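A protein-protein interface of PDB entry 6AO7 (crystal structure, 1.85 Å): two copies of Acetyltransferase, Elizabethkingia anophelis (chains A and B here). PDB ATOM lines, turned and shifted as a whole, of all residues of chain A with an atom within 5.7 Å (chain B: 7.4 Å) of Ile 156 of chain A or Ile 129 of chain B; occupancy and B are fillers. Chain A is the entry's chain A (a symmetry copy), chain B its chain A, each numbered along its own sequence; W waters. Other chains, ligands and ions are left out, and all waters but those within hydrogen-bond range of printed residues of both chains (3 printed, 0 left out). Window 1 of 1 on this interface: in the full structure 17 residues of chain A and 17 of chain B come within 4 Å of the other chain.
N of Ile 156 of chain A is in hydrogen-bond range of O of Thr 111 of chain A (2.7 Å). OD1 of Asn 113 of chain A is in hydrogen-bond range of N of Asp 154 of chain A. OG1 of Thr 130 of chain B lies within hydrogen-bond range of OD2 of Asp 131 of chain B. N of Thr 130 of chain B sits at hydrogen-bond distance from O of Leu 157 of chain B. The side-chain hydroxyl (OG1) of Thr 130 of chain B is in hydrogen-bond range of the side-chain hydroxyl (OG1) of Thr 159 of chain B (2.8 Å). The backbone carbonyl oxygen (O) of Leu 119 of chain B sits at hydrogen-bond distance from the side-chain amide nitrogen (NE2) of Gln 123 of chain B (3.0 Å).
Water W1 lies within hydrogen-bond range of OE1 of Gln 123 of chain B (2.7 Å), ND2 of Asn 113 of chain A (3.2 Å) and O of Phe 127 of chain B (3.4 Å). Water W3 lies within hydrogen-bond range of the backbone carbonyl oxygen of Ile 129 of chain B and the side-chain carboxylate of Asp 154 of chain A. Water W2 lies within hydrogen-bond range of N of Ile 129 of chain B (2.8 Å), OD1 of Asp 154 of chain A (3.0 Å) and OE1 of Gln 123 of chain B (3.4 Å).
Printed residues of chain B that touch a printed residue of chain A: Leu 119, Gln 123, Arg 128, Ile 129, Thr 130, Ile 132 and Ile 156. Along chain B the printed residues that touch a printed residue of chain A span positions 119 to 156. Printed residues of chain A that touch a printed residue of chain B: Asn 113, Leu 119, Ile 129, Ile 132, Asp 154 and Ile 156. Among the printed residues, 9 pairs touch across the chains. Among the printed residues, Asp or Glu carboxylates within 4 Å of a Lys or Arg side-chain nitrogen of the other chain: Asp 154 of chain A with Arg 128 of chain B.
Of chain B, only Ile 129 comes within 4 Å of Ile 156 of chain A. Ile 129 of chain B touches just these residues of chain A: Ile 132 and Ile 156. Printed residues of chain B within 4 Å of Ile 132 of chain A: Ile 129 (3.5 Å), Thr 130 (3.99 Å) and Ile 132 (3.9 Å). Of the printed residues of chain B, Asp 154 of chain A touches Arg 128. Thr 159 of chain B touches none of the printed residues of chain A. The nearest residue of chain A that does not touch Ile 129 of chain B is Asp 154 of chain A (4.2 Å).
Leu 119 of chain A touches its own counterpart, Leu 119 of chain B. Ile 129 of chain A touches Ile 132 of chain B, and with the chains exchanged Ile 132 of chain A touches Ile 129 of chain B. Ile 129 of chain A touches Ile 156 of chain B, and with the chains exchanged Ile 156 of chain A touches Ile 129 of chain B. Ile 132 of chain A touches its own counterpart, Ile 132 of chain B. Of the 9 pairs that touch across the chains among the printed residues, 6 have their exchanged pair printed and touching as well.
Leu 119 of chain A touches Leu 119 of chain B (CD1 to CD1, 3.9 Å). Ile 132 of chain B touches Ile 129 of chain A (CG2 to O, 3.5 Å). Ile 129 of chain A touches Ile 156 of chain B. Ile 132 of chain A touches Ile 129 of chain B. Thr 130 of chain B touches Ile 132 of chain A. Ile 132 of chain A touches Ile 132 of chain B (CD1 to CD1, 3.9 Å). Ile 129 of chain B touches Ile 156 of chain A.
The side-chain amide nitrogen of Asn 113 of chain A is in hydrogen-bond range of the side-chain amide oxygen of Gln 123 of chain B, 2.8 Å away. The side-chain carboxylate (OD2) of Asp 154 of chain A lies within salt-bridge range of the guanidinium group (NH2) of Arg 128 of chain B.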
ATOM      1  N   ILE A 109      -1.659  15.566 -15.170  1.00  0.00           N
ATOM      2  CA  ILE A 109      -1.485  14.125 -15.040  1.00  0.00           C
ATOM      3  C   ILE A 109      -2.735  13.541 -14.400  1.00  0.00           C
ATOM      4  O   ILE A 109      -3.322  14.141 -13.493  1.00  0.00           O
ATOM      5  CB  ILE A 109      -0.215  13.788 -14.243  1.00  0.00           C
ATOM      6  CG1 ILE A 109       0.090  12.288 -14.350  1.00  0.00           C
ATOM      7  CG2 ILE A 109      -0.348  14.272 -12.766  1.00  0.00           C
ATOM      8  CD1 ILE A 109       1.488  11.907 -13.868  1.00  0.00           C
ATOM      9  N   GLY A 110      -3.155  12.378 -14.888  1.00  0.00           N
ATOM     10  CA  GLY A 110      -4.326  11.713 -14.344  1.00  0.00           C
ATOM     11  C   GLY A 110      -4.000  10.340 -13.796  1.00  0.00           C
ATOM     12  O   GLY A 110      -3.342   9.551 -14.474  1.00  0.00           O
ATOM     13  N   THR A 111      -4.433  10.032 -12.579  1.00  0.00           N
ATOM     14  CA  THR A 111      -4.166   8.722 -12.004  1.00  0.00           C
ATOM     15  C   THR A 111      -5.464   8.158 -11.423  1.00  0.00           C
ATOM     16  O   THR A 111      -6.509   8.808 -11.442  1.00  0.00           O
ATOM     17  CB  THR A 111      -3.050   8.794 -10.956  1.00  0.00           C
ATOM     18  OG1 THR A 111      -2.627   7.460 -10.637  1.00  0.00           O
ATOM     19  CG2 THR A 111      -3.556   9.509  -9.677  1.00  0.00           C
ATOM     20  N   GLY A 112      -5.406   6.923 -10.923  1.00  0.00           N
ATOM     21  CA  GLY A 112      -6.610   6.266 -10.454  1.00  0.00           C
ATOM     22  C   GLY A 112      -7.029   6.720  -9.069  1.00  0.00           C
ATOM     23  O   GLY A 112      -6.217   7.162  -8.246  1.00  0.00           O
ATOM     24  N   ASN A 113      -8.335   6.602  -8.795  1.00  0.00           N
ATOM     25  CA  ASN A 113      -8.821   6.979  -7.466  1.00  0.00           C
ATOM     26  C   ASN A 113      -8.158   6.157  -6.362  1.00  0.00           C
ATOM     27  O   ASN A 113      -7.991   6.644  -5.244  1.00  0.00           O
ATOM     28  CB  ASN A 113     -10.346   6.844  -7.386  1.00  0.00           C
ATOM     29  CG  ASN A 113     -10.838   5.450  -7.727  1.00  0.00           C
ATOM     30  OD1 ASN A 113     -11.052   5.129  -8.890  1.00  0.00           O
ATOM     31  ND2 ASN A 113     -11.057   4.624  -6.704  1.00  0.00           N
ATOM     32  N   SER A 114      -7.770   4.926  -6.658  1.00  0.00           N
ATOM     33  CA  SER A 114      -7.150   4.044  -5.676  1.00  0.00           C
ATOM     34  C   SER A 114      -5.654   4.285  -5.510  1.00  0.00           C
ATOM     35  O   SER A 114      -5.050   3.697  -4.604  1.00  0.00           O
ATOM     36  CB  SER A 114      -7.386   2.596  -6.090  1.00  0.00           C
ATOM     37  OG  SER A 114      -7.078   2.445  -7.472  1.00  0.00           O
ATOM     38  N   LEU A 119      -1.019   9.983  -5.564  1.00  0.00           N
ATOM     39  CA  LEU A 119      -1.571  11.305  -5.279  1.00  0.00           C
ATOM     40  C   LEU A 119      -0.639  12.118  -4.381  1.00  0.00           C
ATOM     41  O   LEU A 119      -0.525  13.339  -4.545  1.00  0.00           O
ATOM     42  CB  LEU A 119      -2.951  11.178  -4.644  1.00  0.00           C
ATOM     43  CG  LEU A 119      -4.064  10.635  -5.546  1.00  0.00           C
ATOM     44  CD1 LEU A 119      -5.312  10.457  -4.729  1.00  0.00           C
ATOM     45  CD2 LEU A 119      -4.279  11.583  -6.703  1.00  0.00           C
ATOM     46  N   ILE A 129      -4.782  18.842  -7.136  1.00  0.00           N
ATOM     47  CA  ILE A 129      -5.918  18.050  -7.594  1.00  0.00           C
ATOM     48  C   ILE A 129      -6.977  18.989  -8.165  1.00  0.00           C
ATOM     49  O   ILE A 129      -7.376  19.960  -7.513  1.00  0.00           O
ATOM     50  CB  ILE A 129      -6.466  17.190  -6.451  1.00  0.00           C
ATOM     51  CG1 ILE A 129      -5.382  16.239  -5.939  1.00  0.00           C
ATOM     52  CG2 ILE A 129      -7.697  16.441  -6.903  1.00  0.00           C
ATOM     53  CD1 ILE A 129      -5.853  15.379  -4.791  1.00  0.00           C
ATOM     54  N   ASP A 131      -9.656  17.850 -10.936  1.00  0.00           N
ATOM     55  CA  ASP A 131     -10.815  17.323 -11.651  1.00  0.00           C
ATOM     56  C   ASP A 131     -10.987  15.839 -11.367  1.00  0.00           C
ATOM     57  O   ASP A 131     -10.011  15.117 -11.155  1.00  0.00           O
ATOM     58  CB  ASP A 131     -10.683  17.521 -13.167  1.00  0.00           C
ATOM     59  CG  ASP A 131     -10.740  18.972 -13.579  1.00  0.00           C
ATOM     60  OD1 ASP A 131     -11.864  19.501 -13.706  1.00  0.00           O
ATOM     61  OD2 ASP A 131      -9.662  19.579 -13.776  1.00  0.00           O
ATOM     62  N   ILE A 132     -12.245  15.387 -11.380  1.00  0.00           N
ATOM     63  CA  ILE A 132     -12.576  13.964 -11.319  1.00  0.00           C
ATOM     64  C   ILE A 132     -13.240  13.564 -12.634  1.00  0.00           C
ATOM     65  O   ILE A 132     -14.180  14.228 -13.083  1.00  0.00           O
ATOM     66  CB  ILE A 132     -13.497  13.638 -10.130  1.00  0.00           C
ATOM     67  CG1 ILE A 132     -12.989  14.315  -8.858  1.00  0.00           C
ATOM     68  CG2 ILE A 132     -13.582  12.126  -9.939  1.00  0.00           C
ATOM     69  CD1 ILE A 132     -11.554  13.976  -8.554  1.00  0.00           C
ATOM     70  N   ARG A 133     -12.764  12.483 -13.236  1.00  0.00           N
ATOM     71  CA  ARG A 133     -13.379  11.882 -14.420  1.00  0.00           C
ATOM     72  C   ARG A 133     -14.096  10.603 -13.984  1.00  0.00           C
ATOM     73  O   ARG A 133     -13.492   9.534 -13.923  1.00  0.00           O
ATOM     74  CB  ARG A 133     -12.333  11.582 -15.495  1.00  0.00           C
ATOM     75  CG  ARG A 133     -11.645  12.800 -16.088  1.00  0.00           C
ATOM     76  CD  ARG A 133     -10.645  12.400 -17.175  1.00  0.00           C
ATOM     77  NE  ARG A 133     -10.083  13.554 -17.876  1.00  0.00           N
ATOM     78  CZ  ARG A 133      -9.178  13.471 -18.846  1.00  0.00           C
ATOM     79  NH1 ARG A 133      -8.730  12.285 -19.236  1.00  0.00           N
ATOM     80  NH2 ARG A 133      -8.719  14.572 -19.425  1.00  0.00           N
ATOM     81  N   PHE A 137     -11.931   4.813 -16.001  1.00  0.00           N
ATOM     82  CA  PHE A 137     -11.297   3.513 -16.187  1.00  0.00           C
ATOM     83  C   PHE A 137     -12.329   2.442 -16.507  1.00  0.00           C
ATOM     84  O   PHE A 137     -12.071   1.547 -17.323  1.00  0.00           O
ATOM     85  CB  PHE A 137     -10.482   3.147 -14.950  1.00  0.00           C
ATOM     86  CG  PHE A 137      -9.250   3.995 -14.767  1.00  0.00           C
ATOM     87  CD1 PHE A 137      -8.115   3.759 -15.528  1.00  0.00           C
ATOM     88  CD2 PHE A 137      -9.227   5.021 -13.846  1.00  0.00           C
ATOM     89  CE1 PHE A 137      -6.979   4.531 -15.372  1.00  0.00           C
ATOM     90  CE2 PHE A 137      -8.088   5.807 -13.680  1.00  0.00           C
ATOM     91  CZ  PHE A 137      -6.960   5.553 -14.447  1.00  0.00           C
ATOM     92  N   ASP A 154     -12.378   5.681 -11.332  1.00  0.00           N
ATOM     93  CA  ASP A 154     -12.398   7.077 -11.737  1.00  0.00           C
ATOM     94  C   ASP A 154     -10.978   7.596 -11.900  1.00  0.00           C
ATOM     95  O   ASP A 154     -10.039   7.105 -11.270  1.00  0.00           O
ATOM     96  CB  ASP A 154     -13.144   7.938 -10.707  1.00  0.00           C
ATOM     97  CG  ASP A 154     -14.460   7.320 -10.258  1.00  0.00           C
ATOM     98  OD1 ASP A 154     -14.761   7.372  -9.045  1.00  0.00           O
ATOM     99  OD2 ASP A 154     -15.205   6.774 -11.102  1.00  0.00           O
ATOM    100  N   MET A 155     -10.809   8.588 -12.768  1.00  0.00           N
ATOM    101  CA  MET A 155      -9.516   9.234 -12.916  1.00  0.00           C
ATOM    102  C   MET A 155      -9.502  10.519 -12.101  1.00  0.00           C
ATOM    103  O   MET A 155     -10.436  11.322 -12.190  1.00  0.00           O
ATOM    104  CB  MET A 155      -9.193   9.542 -14.375  1.00  0.00           C
ATOM    105  CG  MET A 155      -8.053  10.513 -14.485  1.00  0.00           C
ATOM    106  SD  MET A 155      -7.512  10.732 -16.173  1.00  0.00           S
ATOM    107  CE  MET A 155      -6.606   9.194 -16.375  1.00  0.00           C
ATOM    108  N   ILE A 156      -8.456  10.693 -11.293  1.00  0.00           N
ATOM    109  CA  ILE A 156      -8.189  11.948 -10.603  1.00  0.00           C
ATOM    110  C   ILE A 156      -7.200  12.740 -11.433  1.00  0.00           C
ATOM    111  O   ILE A 156      -6.088  12.269 -11.703  1.00  0.00           O
ATOM    112  CB  ILE A 156      -7.635  11.706  -9.193  1.00  0.00           C
ATOM    113  CG1 ILE A 156      -8.580  10.803  -8.420  1.00  0.00           C
ATOM    114  CG2 ILE A 156      -7.399  13.037  -8.493  1.00  0.00           C
ATOM    115  CD1 ILE A 156      -7.987  10.352  -7.111  1.00  0.00           C
ATOM    116  N   LEU A 157      -7.595  13.936 -11.855  1.00  0.00           N
ATOM    117  CA  LEU A 157      -6.752  14.768 -12.704  1.00  0.00           C
ATOM    118  C   LEU A 157      -6.085  15.832 -11.844  1.00  0.00           C
ATOM    119  O   LEU A 157      -6.761  16.518 -11.073  1.00  0.00           O
ATOM    120  CB  LEU A 157      -7.589  15.416 -13.812  1.00  0.00           C
ATOM    121  CG  LEU A 157      -6.975  15.681 -15.190  1.00  0.00           C
ATOM    122  CD1 LEU A 157      -6.655  14.378 -15.907  1.00  0.00           C
ATOM    123  CD2 LEU A 157      -7.889  16.543 -16.039  1.00  0.00           C
ATOM    124  N   LEU A 158      -4.770  15.969 -11.979  1.00  0.00           N
ATOM    125  CA  LEU A 158      -4.008  16.985 -11.269  1.00  0.00           C
ATOM    126  C   LEU A 158      -3.334  17.905 -12.274  1.00  0.00           C
ATOM    127  O   LEU A 158      -2.953  17.480 -13.361  1.00  0.00           O
ATOM    128  CB  LEU A 158      -2.935  16.374 -10.347  1.00  0.00           C
ATOM    129  CG  LEU A 158      -3.373  15.320  -9.331  1.00  0.00           C
ATOM    130  CD1 LEU A 158      -3.296  13.907  -9.920  1.00  0.00           C
ATOM    131  CD2 LEU A 158      -2.496  15.404  -8.051  1.00  0.00           C
ATOM    132  N   LEU B 119      -7.936   9.328   2.177  1.00  0.00           N
ATOM    133  CA  LEU B 119      -8.587   9.031   0.904  1.00  0.00           C
ATOM    134  C   LEU B 119      -8.705   7.524   0.675  1.00  0.00           C
ATOM    135  O   LEU B 119      -9.703   7.057   0.113  1.00  0.00           O
ATOM    136  CB  LEU B 119      -7.832   9.690  -0.244  1.00  0.00           C
ATOM    137  CG  LEU B 119      -7.878  11.220  -0.294  1.00  0.00           C
ATOM    138  CD1 LEU B 119      -6.985  11.701  -1.403  1.00  0.00           C
ATOM    139  CD2 LEU B 119      -9.307  11.673  -0.488  1.00  0.00           C
ATOM    140  N   TYR B 120      -7.712   6.745   1.119  1.00  0.00           N
ATOM    141  CA  TYR B 120      -7.855   5.290   1.085  1.00  0.00           C
ATOM    142  C   TYR B 120      -9.017   4.834   1.957  1.00  0.00           C
ATOM    143  O   TYR B 120      -9.903   4.102   1.497  1.00  0.00           O
ATOM    144  CB  TYR B 120      -6.570   4.601   1.550  1.00  0.00           C
ATOM    145  CG  TYR B 120      -6.842   3.167   1.989  1.00  0.00           C
ATOM    146  CD1 TYR B 120      -6.930   2.136   1.058  1.00  0.00           C
ATOM    147  CD2 TYR B 120      -7.033   2.857   3.331  1.00  0.00           C
ATOM    148  CE1 TYR B 120      -7.197   0.828   1.463  1.00  0.00           C
ATOM    149  CE2 TYR B 120      -7.308   1.557   3.745  1.00  0.00           C
ATOM    150  CZ  TYR B 120      -7.396   0.556   2.805  1.00  0.00           C
ATOM    151  OH  TYR B 120      -7.660  -0.726   3.237  1.00  0.00           O
ATOM    152  N   GLN B 123     -12.647   5.470   0.825  1.00  0.00           N
ATOM    153  CA  GLN B 123     -12.986   4.672  -0.351  1.00  0.00           C
ATOM    154  C   GLN B 123     -13.160   3.202   0.001  1.00  0.00           C
ATOM    155  O   GLN B 123     -14.027   2.525  -0.568  1.00  0.00           O
ATOM    156  CB  GLN B 123     -11.921   4.834  -1.431  1.00  0.00           C
ATOM    157  CG  GLN B 123     -11.891   6.234  -1.988  1.00  0.00           C
ATOM    158  CD  GLN B 123     -10.950   6.305  -3.154  1.00  0.00           C
ATOM    159  OE1 GLN B 123     -11.281   5.862  -4.246  1.00  0.00           O
ATOM    160  NE2 GLN B 123      -9.755   6.833  -2.923  1.00  0.00           N
ATOM    161  N   GLY B 126     -16.666   2.699   0.861  1.00  0.00           N
ATOM    162  CA  GLY B 126     -17.688   2.885  -0.153  1.00  0.00           C
ATOM    163  C   GLY B 126     -17.822   4.287  -0.691  1.00  0.00           C
ATOM    164  O   GLY B 126     -18.666   4.515  -1.565  1.00  0.00           O
ATOM    165  N   PHE B 127     -17.026   5.234  -0.217  1.00  0.00           N
ATOM    166  CA  PHE B 127     -17.097   6.599  -0.718  1.00  0.00           C
ATOM    167  C   PHE B 127     -16.349   6.709  -2.036  1.00  0.00           C
ATOM    168  O   PHE B 127     -15.261   6.159  -2.191  1.00  0.00           O
ATOM    169  CB  PHE B 127     -16.493   7.566   0.295  1.00  0.00           C
ATOM    170  CG  PHE B 127     -17.323   7.776   1.503  1.00  0.00           C
ATOM    171  CD1 PHE B 127     -17.221   6.930   2.614  1.00  0.00           C
ATOM    172  CD2 PHE B 127     -18.201   8.847   1.557  1.00  0.00           C
ATOM    173  CE1 PHE B 127     -17.991   7.156   3.747  1.00  0.00           C
ATOM    174  CE2 PHE B 127     -18.971   9.067   2.680  1.00  0.00           C
ATOM    175  CZ  PHE B 127     -18.867   8.221   3.781  1.00  0.00           C
ATOM    176  N   ARG B 128     -16.945   7.415  -2.992  1.00  0.00           N
ATOM    177  CA  ARG B 128     -16.301   7.705  -4.269  1.00  0.00           C
ATOM    178  C   ARG B 128     -15.822   9.148  -4.257  1.00  0.00           C
ATOM    179  O   ARG B 128     -16.500  10.024  -3.719  1.00  0.00           O
ATOM    180  CB  ARG B 128     -17.272   7.500  -5.437  1.00  0.00           C
ATOM    181  CG  ARG B 128     -17.829   6.090  -5.571  1.00  0.00           C
ATOM    182  CD  ARG B 128     -16.951   5.192  -6.435  1.00  0.00           C
ATOM    183  NE  ARG B 128     -16.854   5.637  -7.828  1.00  0.00           N
ATOM    184  CZ  ARG B 128     -17.695   5.279  -8.796  1.00  0.00           C
ATOM    185  NH1 ARG B 128     -18.712   4.475  -8.530  1.00  0.00           N
ATOM    186  NH2 ARG B 128     -17.519   5.729 -10.037  1.00  0.00           N
ATOM    187  N   ILE B 129     -14.672   9.413  -4.875  1.00  0.00           N
ATOM    188  CA  ILE B 129     -14.234  10.799  -4.990  1.00  0.00           C
ATOM    189  C   ILE B 129     -15.115  11.512  -6.012  1.00  0.00           C
ATOM    190  O   ILE B 129     -15.291  11.032  -7.136  1.00  0.00           O
ATOM    191  CB  ILE B 129     -12.750  10.861  -5.364  1.00  0.00           C
ATOM    192  CG1 ILE B 129     -11.905  10.170  -4.291  1.00  0.00           C
ATOM    193  CG2 ILE B 129     -12.323  12.295  -5.572  1.00  0.00           C
ATOM    194  CD1 ILE B 129     -10.431  10.175  -4.615  1.00  0.00           C
ATOM    195  N   THR B 130     -15.719  12.641  -5.615  1.00  0.00           N
ATOM    196  CA  THR B 130     -16.669  13.265  -6.540  1.00  0.00           C
ATOM    197  C   THR B 130     -16.414  14.735  -6.854  1.00  0.00           C
ATOM    198  O   THR B 130     -16.826  15.204  -7.922  1.00  0.00           O
ATOM    199  CB  THR B 130     -18.108  13.122  -6.035  1.00  0.00           C
ATOM    200  OG1 THR B 130     -18.229  13.639  -4.700  1.00  0.00           O
ATOM    201  CG2 THR B 130     -18.554  11.659  -6.093  1.00  0.00           C
ATOM    202  N   ASP B 131     -15.756  15.480  -5.968  1.00  0.00           N
ATOM    203  CA  ASP B 131     -15.678  16.927  -6.141  1.00  0.00           C
ATOM    204  C   ASP B 131     -14.401  17.471  -5.519  1.00  0.00           C
ATOM    205  O   ASP B 131     -13.907  16.940  -4.521  1.00  0.00           O
ATOM    206  CB  ASP B 131     -16.878  17.639  -5.502  1.00  0.00           C
ATOM    207  CG  ASP B 131     -18.180  17.347  -6.207  1.00  0.00           C
ATOM    208  OD1 ASP B 131     -18.456  18.009  -7.228  1.00  0.00           O
ATOM    209  OD2 ASP B 131     -18.926  16.456  -5.736  1.00  0.00           O
ATOM    210  N   ILE B 132     -13.880  18.550  -6.108  1.00  0.00           N
ATOM    211  CA  ILE B 132     -12.773  19.312  -5.533  1.00  0.00           C
ATOM    212  C   ILE B 132     -13.278  20.708  -5.179  1.00  0.00           C
ATOM    213  O   ILE B 132     -13.900  21.375  -6.012  1.00  0.00           O
ATOM    214  CB  ILE B 132     -11.574  19.402  -6.494  1.00  0.00           C
ATOM    215  CG1 ILE B 132     -11.269  18.032  -7.098  1.00  0.00           C
ATOM    216  CG2 ILE B 132     -10.356  19.948  -5.754  1.00  0.00           C
ATOM    217  CD1 ILE B 132     -11.060  16.970  -6.051  1.00  0.00           C
ATOM    218  N   ILE B 156     -11.121  17.666  -0.817  1.00  0.00           N
ATOM    219  CA  ILE B 156     -11.583  16.578  -1.669  1.00  0.00           C
ATOM    220  C   ILE B 156     -12.879  16.047  -1.090  1.00  0.00           C
ATOM    221  O   ILE B 156     -12.914  15.601   0.064  1.00  0.00           O
ATOM    222  CB  ILE B 156     -10.538  15.458  -1.766  1.00  0.00           C
ATOM    223  CG1 ILE B 156      -9.211  16.035  -2.225  1.00  0.00           C
ATOM    224  CG2 ILE B 156     -11.044  14.356  -2.687  1.00  0.00           C
ATOM    225  CD1 ILE B 156      -8.094  15.030  -2.129  1.00  0.00           C
ATOM    226  N   LEU B 157     -13.950  16.100  -1.874  1.00  0.00           N
ATOM    227  CA  LEU B 157     -15.262  15.668  -1.410  1.00  0.00           C
ATOM    228  C   LEU B 157     -15.541  14.272  -1.950  1.00  0.00           C
ATOM    229  O   LEU B 157     -15.387  14.031  -3.150  1.00  0.00           O
ATOM    230  CB  LEU B 157     -16.341  16.651  -1.874  1.00  0.00           C
ATOM    231  CG  LEU B 157     -17.575  16.915  -1.005  1.00  0.00           C
ATOM    232  CD1 LEU B 157     -17.195  17.621   0.287  1.00  0.00           C
ATOM    233  CD2 LEU B 157     -18.615  17.718  -1.762  1.00  0.00           C
ATOM    234  N   LEU B 158     -15.949  13.363  -1.071  1.00  0.00           N
ATOM    235  CA  LEU B 158     -16.311  12.007  -1.452  1.00  0.00           C
ATOM    236  C   LEU B 158     -17.765  11.751  -1.087  1.00  0.00           C
ATOM    237  O   LEU B 158     -18.270  12.282  -0.103  1.00  0.00           O
ATOM    238  CB  LEU B 158     -15.426  10.950  -0.765  1.00  0.00           C
ATOM    239  CG  LEU B 158     -13.909  11.084  -0.896  1.00  0.00           C
ATOM    240  CD1 LEU B 158     -13.322  11.932   0.239  1.00  0.00           C
ATOM    241  CD2 LEU B 158     -13.239   9.683  -0.905  1.00  0.00           C
ATOM    242  N   THR B 159     -18.421  10.900  -1.871  1.00  0.00           N
ATOM    243  CA  THR B 159     -19.857  10.707  -1.784  1.00  0.00           C
ATOM    244  C   THR B 159     -20.171   9.231  -1.848  1.00  0.00           C
ATOM    245  O   THR B 159     -19.618   8.506  -2.676  1.00  0.00           O
ATOM    246  CB  THR B 159     -20.614  11.398  -2.923  1.00  0.00           C
ATOM    247  OG1 THR B 159     -20.277  12.788  -2.952  1.00  0.00           O
ATOM    248  CG2 THR B 159     -22.107  11.243  -2.726  1.00  0.00           C
HETATM  249  O   HOH W   1     -13.692   4.922  -4.980  1.00  0.00           O
HETATM  250  O   HOH W   2     -13.518   7.382  -6.356  1.00  0.00           O
HETATM  251  O   HOH W   3     -16.835   9.509  -8.748  1.00  0.00           O
